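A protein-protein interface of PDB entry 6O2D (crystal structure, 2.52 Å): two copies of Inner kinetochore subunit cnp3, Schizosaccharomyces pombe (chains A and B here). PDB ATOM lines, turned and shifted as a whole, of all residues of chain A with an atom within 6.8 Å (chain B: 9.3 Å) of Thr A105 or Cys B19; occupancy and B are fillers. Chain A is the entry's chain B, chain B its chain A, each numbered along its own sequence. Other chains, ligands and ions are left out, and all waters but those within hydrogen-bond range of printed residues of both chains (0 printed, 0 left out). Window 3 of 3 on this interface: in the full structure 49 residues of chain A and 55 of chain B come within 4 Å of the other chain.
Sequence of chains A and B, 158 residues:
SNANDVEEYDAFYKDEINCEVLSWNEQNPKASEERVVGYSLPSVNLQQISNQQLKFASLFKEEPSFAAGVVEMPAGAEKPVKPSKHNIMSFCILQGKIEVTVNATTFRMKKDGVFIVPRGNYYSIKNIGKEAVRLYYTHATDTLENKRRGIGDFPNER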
ATOM      1  N   VAL A 100       5.691 -33.562  12.396  1.00  0.00           N
ATOM      2  CA  VAL A 100       4.470 -33.145  13.059  1.00  0.00           C
ATOM      3  C   VAL A 100       3.754 -32.070  12.244  1.00  0.00           C
ATOM      4  O   VAL A 100       4.393 -31.189  11.658  1.00  0.00           O
ATOM      5  CB  VAL A 100       4.775 -32.693  14.503  1.00  0.00           C
ATOM      6  CG1 VAL A 100       5.969 -31.784  14.511  1.00  0.00           C
ATOM      7  CG2 VAL A 100       3.572 -32.011  15.120  1.00  0.00           C
ATOM      8  N   THR A 101       2.424 -32.203  12.165  1.00  0.00           N
ATOM      9  CA  THR A 101       1.483 -31.221  11.625  1.00  0.00           C
ATOM     10  C   THR A 101       0.716 -30.491  12.709  1.00  0.00           C
ATOM     11  O   THR A 101       0.050 -31.116  13.550  1.00  0.00           O
ATOM     12  CB  THR A 101       0.487 -31.815  10.622  1.00  0.00           C
ATOM     13  OG1 THR A 101       1.063 -32.867   9.825  1.00  0.00           O
ATOM     14  CG2 THR A 101      -0.468 -30.739   9.952  1.00  0.00           C
ATOM     15  N   VAL A 102       0.814 -29.163  12.663  1.00  0.00           N
ATOM     16  CA  VAL A 102      -0.048 -28.286  13.432  1.00  0.00           C
ATOM     17  C   VAL A 102      -0.767 -27.413  12.420  1.00  0.00           C
ATOM     18  O   VAL A 102      -0.156 -26.512  11.836  1.00  0.00           O
ATOM     19  CB  VAL A 102       0.733 -27.428  14.441  1.00  0.00           C
ATOM     20  CG1 VAL A 102      -0.206 -26.503  15.202  1.00  0.00           C
ATOM     21  CG2 VAL A 102       1.527 -28.298  15.375  1.00  0.00           C
ATOM     22  N   ASN A 103      -2.063 -27.674  12.210  1.00  0.00           N
ATOM     23  CA  ASN A 103      -2.926 -26.843  11.354  1.00  0.00           C
ATOM     24  C   ASN A 103      -2.401 -26.723   9.921  1.00  0.00           C
ATOM     25  O   ASN A 103      -2.261 -25.626   9.373  1.00  0.00           O
ATOM     26  CB  ASN A 103      -3.145 -25.459  11.971  1.00  0.00           C
ATOM     27  CG  ASN A 103      -4.083 -25.508  13.157  1.00  0.00           C
ATOM     28  OD1 ASN A 103      -4.709 -26.542  13.425  1.00  0.00           O
ATOM     29  ND2 ASN A 103      -4.195 -24.397  13.873  1.00  0.00           N
ATOM     30  N   ALA A 104      -2.114 -27.869   9.310  1.00  0.00           N
ATOM     31  CA  ALA A 104      -1.695 -27.984   7.915  1.00  0.00           C
ATOM     32  C   ALA A 104      -0.361 -27.300   7.623  1.00  0.00           C
ATOM     33  O   ALA A 104      -0.017 -27.106   6.451  1.00  0.00           O
ATOM     34  CB  ALA A 104      -2.774 -27.457   6.954  1.00  0.00           C
ATOM     35  N   THR A 105       0.405 -26.939   8.649  1.00  0.00           N
ATOM     36  CA  THR A 105       1.800 -26.540   8.503  1.00  0.00           C
ATOM     37  C   THR A 105       2.638 -27.651   9.127  1.00  0.00           C
ATOM     38  O   THR A 105       2.416 -28.012  10.287  1.00  0.00           O
ATOM     39  CB  THR A 105       2.075 -25.196   9.188  1.00  0.00           C
ATOM     40  OG1 THR A 105       1.430 -24.129   8.473  1.00  0.00           O
ATOM     41  CG2 THR A 105       3.565 -24.936   9.255  1.00  0.00           C
ATOM     42  N   THR A 106       3.575 -28.207   8.357  1.00  0.00           N
ATOM     43  CA  THR A 106       4.333 -29.394   8.749  1.00  0.00           C
ATOM     44  C   THR A 106       5.819 -29.098   8.943  1.00  0.00           C
ATOM     45  O   THR A 106       6.409 -28.293   8.210  1.00  0.00           O
ATOM     46  CB  THR A 106       4.139 -30.494   7.700  1.00  0.00           C
ATOM     47  OG1 THR A 106       2.739 -30.762   7.559  1.00  0.00           O
ATOM     48  CG2 THR A 106       4.857 -31.759   8.099  1.00  0.00           C
ATOM     49  N   PHE A 107       6.403 -29.734   9.962  1.00  0.00           N
ATOM     50  CA  PHE A 107       7.796 -29.549  10.347  1.00  0.00           C
ATOM     51  C   PHE A 107       8.332 -30.841  10.955  1.00  0.00           C
ATOM     52  O   PHE A 107       7.570 -31.656  11.473  1.00  0.00           O
ATOM     53  CB  PHE A 107       7.948 -28.404  11.367  1.00  0.00           C
ATOM     54  CG  PHE A 107       7.066 -28.535  12.608  1.00  0.00           C
ATOM     55  CD1 PHE A 107       5.681 -28.542  12.517  1.00  0.00           C
ATOM     56  CD2 PHE A 107       7.634 -28.636  13.871  1.00  0.00           C
ATOM     57  CE1 PHE A 107       4.883 -28.668  13.672  1.00  0.00           C
ATOM     58  CE2 PHE A 107       6.839 -28.736  15.013  1.00  0.00           C
ATOM     59  CZ  PHE A 107       5.470 -28.756  14.914  1.00  0.00           C
ATOM     60  N   LYS B  14      14.389 -26.548  11.047  1.00  0.00           N
ATOM     61  CA  LYS B  14      14.194 -25.110  11.218  1.00  0.00           C
ATOM     62  C   LYS B  14      14.395 -24.696  12.674  1.00  0.00           C
ATOM     63  O   LYS B  14      14.063 -25.434  13.606  1.00  0.00           O
ATOM     64  CB  LYS B  14      12.796 -24.692  10.741  1.00  0.00           C
ATOM     65  CG  LYS B  14      12.745 -24.280   9.265  1.00  0.00           C
ATOM     66  CD  LYS B  14      11.372 -23.754   8.831  1.00  0.00           C
ATOM     67  CE  LYS B  14      11.056 -22.358   9.370  1.00  0.00           C
ATOM     68  NZ  LYS B  14      12.076 -21.340   9.010  1.00  0.00           N
ATOM     69  N   GLU B  16      13.259 -21.571  14.159  1.00  0.00           N
ATOM     70  CA  GLU B  16      11.973 -21.070  14.613  1.00  0.00           C
ATOM     71  C   GLU B  16      10.926 -21.547  13.626  1.00  0.00           C
ATOM     72  O   GLU B  16      11.169 -21.567  12.416  1.00  0.00           O
ATOM     73  CB  GLU B  16      11.951 -19.535  14.685  1.00  0.00           C
ATOM     74  CG  GLU B  16      12.471 -18.923  15.981  1.00  0.00           C
ATOM     75  CD  GLU B  16      12.277 -17.408  16.034  1.00  0.00           C
ATOM     76  OE1 GLU B  16      11.420 -16.889  15.283  1.00  0.00           O
ATOM     77  OE2 GLU B  16      12.973 -16.736  16.828  1.00  0.00           O
ATOM     78  N   ILE B  17       9.768 -21.950  14.136  1.00  0.00           N
ATOM     79  CA  ILE B  17       8.688 -22.443  13.292  1.00  0.00           C
ATOM     80  C   ILE B  17       7.475 -21.562  13.531  1.00  0.00           C
ATOM     81  O   ILE B  17       6.866 -21.594  14.609  1.00  0.00           O
ATOM     82  CB  ILE B  17       8.391 -23.920  13.555  1.00  0.00           C
ATOM     83  CG1 ILE B  17       9.734 -24.644  13.675  1.00  0.00           C
ATOM     84  CG2 ILE B  17       7.510 -24.489  12.447  1.00  0.00           C
ATOM     85  CD1 ILE B  17       9.664 -26.113  13.757  1.00  0.00           C
ATOM     86  N   ASN B  18       7.131 -20.776  12.523  1.00  0.00           N
ATOM     87  CA  ASN B  18       5.934 -19.963  12.543  1.00  0.00           C
ATOM     88  C   ASN B  18       4.795 -20.710  11.866  1.00  0.00           C
ATOM     89  O   ASN B  18       5.006 -21.517  10.955  1.00  0.00           O
ATOM     90  CB  ASN B  18       6.179 -18.624  11.854  1.00  0.00           C
ATOM     91  CG  ASN B  18       5.276 -17.536  12.381  1.00  0.00           C
ATOM     92  OD1 ASN B  18       4.069 -17.730  12.518  1.00  0.00           O
ATOM     93  ND2 ASN B  18       5.857 -16.384  12.696  1.00  0.00           N
ATOM     94  N   CYS B  19       3.581 -20.434  12.327  1.00  0.00           N
ATOM     95  CA  CYS B  19       2.413 -21.167  11.873  1.00  0.00           C
ATOM     96  C   CYS B  19       1.172 -20.314  12.086  1.00  0.00           C
ATOM     97  O   CYS B  19       1.147 -19.434  12.949  1.00  0.00           O
ATOM     98  CB  CYS B  19       2.292 -22.494  12.628  1.00  0.00           C
ATOM     99  SG  CYS B  19       0.907 -23.553  12.169  1.00  0.00           S
ATOM    100  N   GLU B  20       0.152 -20.572  11.269  1.00  0.00           N
ATOM    101  CA  GLU B  20      -1.136 -19.903  11.397  1.00  0.00           C
ATOM    102  C   GLU B  20      -2.018 -20.742  12.317  1.00  0.00           C
ATOM    103  O   GLU B  20      -2.236 -21.926  12.052  1.00  0.00           O
ATOM    104  CB  GLU B  20      -1.787 -19.724  10.025  1.00  0.00           C
ATOM    105  CG  GLU B  20      -2.896 -18.675   9.976  1.00  0.00           C
ATOM    106  CD  GLU B  20      -3.764 -18.799   8.728  1.00  0.00           C
ATOM    107  OE1 GLU B  20      -4.892 -19.328   8.833  1.00  0.00           O
ATOM    108  OE2 GLU B  20      -3.318 -18.380   7.638  1.00  0.00           O
ATOM    109  N   VAL B  21      -2.518 -20.143  13.400  1.00  0.00           N
ATOM    110  CA  VAL B  21      -3.264 -20.884  14.409  1.00  0.00           C
ATOM    111  C   VAL B  21      -4.579 -20.178  14.692  1.00  0.00           C
ATOM    112  O   VAL B  21      -4.677 -18.948  14.616  1.00  0.00           O
ATOM    113  CB  VAL B  21      -2.454 -21.054  15.722  1.00  0.00           C
ATOM    114  CG1 VAL B  21      -1.143 -21.800  15.467  1.00  0.00           C
ATOM    115  CG2 VAL B  21      -2.198 -19.710  16.392  1.00  0.00           C
ATOM    116  N   LEU B  22      -5.596 -20.963  15.045  1.00  0.00           N
ATOM    117  CA  LEU B  22      -6.863 -20.375  15.467  1.00  0.00           C
ATOM    118  C   LEU B  22      -6.752 -19.879  16.895  1.00  0.00           C
ATOM    119  O   LEU B  22      -5.929 -20.342  17.674  1.00  0.00           O
ATOM    120  CB  LEU B  22      -8.029 -21.359  15.335  1.00  0.00           C
ATOM    121  CG  LEU B  22      -8.463 -21.575  13.884  1.00  0.00           C
ATOM    122  CD1 LEU B  22      -7.642 -22.705  13.272  1.00  0.00           C
ATOM    123  CD2 LEU B  22      -9.962 -21.842  13.743  1.00  0.00           C
ATOM    124  N   SER B  32      -7.743 -15.914  13.640  1.00  0.00           N
ATOM    125  CA  SER B  32      -6.511 -16.682  13.521  1.00  0.00           C
ATOM    126  C   SER B  32      -5.302 -15.779  13.658  1.00  0.00           C
ATOM    127  O   SER B  32      -5.392 -14.562  13.501  1.00  0.00           O
ATOM    128  CB  SER B  32      -6.425 -17.416  12.185  1.00  0.00           C
ATOM    129  OG  SER B  32      -7.239 -18.573  12.199  1.00  0.00           O
ATOM    130  N   GLU B  33      -4.142 -16.394  13.888  1.00  0.00           N
ATOM    131  CA  GLU B  33      -2.951 -15.573  14.005  1.00  0.00           C
ATOM    132  C   GLU B  33      -1.740 -16.223  13.365  1.00  0.00           C
ATOM    133  O   GLU B  33      -1.724 -17.391  12.980  1.00  0.00           O
ATOM    134  CB  GLU B  33      -2.381 -15.318  15.407  1.00  0.00           C
ATOM    135  CG  GLU B  33      -3.119 -15.239  16.673  1.00  0.00           C
ATOM    136  CD  GLU B  33      -2.053 -14.752  17.674  1.00  0.00           C
ATOM    137  OE1 GLU B  33      -1.093 -14.032  17.252  1.00  0.00           O
ATOM    138  OE2 GLU B  33      -2.010 -15.343  18.790  1.00  0.00           O
ATOM    139  N   GLU B  34      -0.726 -15.380  13.317  1.00  0.00           N
ATOM    140  CA  GLU B  34       0.671 -15.684  13.088  1.00  0.00           C
ATOM    141  C   GLU B  34       1.291 -15.886  14.474  1.00  0.00           C
ATOM    142  O   GLU B  34       1.229 -14.972  15.299  1.00  0.00           O
ATOM    143  CB  GLU B  34       1.219 -14.412  12.443  1.00  0.00           C
ATOM    144  CG  GLU B  34       0.910 -14.138  10.963  1.00  0.00           C
ATOM    145  CD  GLU B  34       2.157 -13.769  10.155  1.00  0.00           C
ATOM    146  OE1 GLU B  34       3.265 -13.711  10.753  1.00  0.00           O
ATOM    147  OE2 GLU B  34       2.047 -13.513   8.937  1.00  0.00           O
ATOM    148  N   ARG B  35       1.840 -17.068  14.779  1.00  0.00           N
ATOM    149  CA  ARG B  35       2.613 -17.190  16.019  1.00  0.00           C
ATOM    150  C   ARG B  35       3.667 -18.294  15.905  1.00  0.00           C
ATOM    151  O   ARG B  35       3.473 -19.315  15.229  1.00  0.00           O
ATOM    152  CB  ARG B  35       1.744 -17.419  17.278  1.00  0.00           C
ATOM    153  CG  ARG B  35       1.125 -18.795  17.529  1.00  0.00           C
ATOM    154  CD  ARG B  35       0.338 -18.810  18.878  1.00  0.00           C
ATOM    155  NE  ARG B  35       1.192 -18.750  20.070  1.00  0.00           N
ATOM    156  CZ  ARG B  35       0.753 -18.524  21.309  1.00  0.00           C
ATOM    157  NH1 ARG B  35      -0.538 -18.325  21.533  1.00  0.00           N
ATOM    158  NH2 ARG B  35       1.608 -18.489  22.326  1.00  0.00           N
ATOM    159  N   VAL B  36       4.785 -18.078  16.600  1.00  0.00           N
ATOM    160  CA  VAL B  36       5.880 -19.044  16.643  1.00  0.00           C
ATOM    161  C   VAL B  36       5.447 -20.208  17.531  1.00  0.00           C
ATOM    162  O   VAL B  36       5.262 -20.041  18.740  1.00  0.00           O
ATOM    163  CB  VAL B  36       7.177 -18.404  17.156  1.00  0.00           C
ATOM    164  CG1 VAL B  36       8.353 -19.350  16.962  1.00  0.00           C
ATOM    165  CG2 VAL B  36       7.437 -17.081  16.449  1.00  0.00           C
ATOM    166  N   VAL B  37       5.258 -21.387  16.935  1.00  0.00           N
ATOM    167  CA  VAL B  37       4.760 -22.544  17.673  1.00  0.00           C
ATOM    168  C   VAL B  37       5.826 -23.618  17.852  1.00  0.00           C
ATOM    169  O   VAL B  37       5.521 -24.703  18.360  1.00  0.00           O
ATOM    170  CB  VAL B  37       3.504 -23.142  17.019  1.00  0.00           C
ATOM    171  CG1 VAL B  37       2.412 -22.094  16.914  1.00  0.00           C
ATOM    172  CG2 VAL B  37       3.846 -23.753  15.665  1.00  0.00           C
ATOM    173  N   GLY B  38       7.067 -23.350  17.456  1.00  0.00           N
ATOM    174  CA  GLY B  38       8.110 -24.343  17.611  1.00  0.00           C
ATOM    175  C   GLY B  38       9.500 -23.747  17.605  1.00  0.00           C
ATOM    176  O   GLY B  38       9.790 -22.813  16.850  1.00  0.00           O
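No position is printed for both chains.
Thr A101 touches none of the printed residues of chain B.
Of chain B, only Cys B19 (3.6 Å) comes within 4 Å of Thr A105.
Thr A106 touches none of the printed residues of chain B.
Of the printed residues of chain B, Phe A107 touches Ile B17 (3.2 Å).
Of the printed residues of chain A, Ile B17 touches Phe A107 (3.2 Å).
Cys B19 touches two residues of chain A.
Of the printed residues of chain A, Val B21 touches Asn A103.
Printed residues of chain A within 4 Å of Leu B22: Asn A103.
Glu B33 touches none of the printed residues of chain A.
The nearest residue of chain B that does not touch Thr A105 is Asn B18 (4.1 Å).
Of the 8 printed residues of chain A, 4 touch a printed residue of chain B.
Printed residues of chain B that touch a printed residue of chain A: Ile B17, Cys B19, Glu B20, Val B21 and Leu B22.
Along chain B the printed residues that touch a printed residue of chain A span positions 17 to 22.
Among the printed residues, 6 pairs touch across the chains.
Among the printed residues, no Asp or Glu carboxylate lies within 4 Å of a Lys or Arg side-chain nitrogen of the other chain.
Among the printed residues, pairs that only touch across the chains: Phe A107 with Ile B17, Asn A103 with Glu B20, Asn A103 with Val B21 and Asn A103 with Leu B22.
The side-chain sulfur of Cys B19 lies close to the side-chain hydroxyl of Thr A105, 3.8 Å away.
The backbone carbonyl oxygen (O) of Val A102 sits at hydrogen-bond distance from the side-chain sulfur (SG) of Cys B19 (3.2 Å).
O of Cys B19 lies within hydrogen-bond range of N of Arg B35.
The backbone carbonyl oxygen of Gly B38 lies within hydrogen-bond range of the backbone NH of Ile B17, 2.8 Å away.
The backbone NH of Val A100 is in hydrogen-bond range of the backbone carbonyl oxygen of Phe A107, 2.8 Å away.
The backbone carbonyl oxygen of Ile B17 is in hydrogen-bond range of the backbone NH of Val B37, 2.8 Å away.
O of Val B21 is in hydrogen-bond range of N of Glu B33 (2.7 Å).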
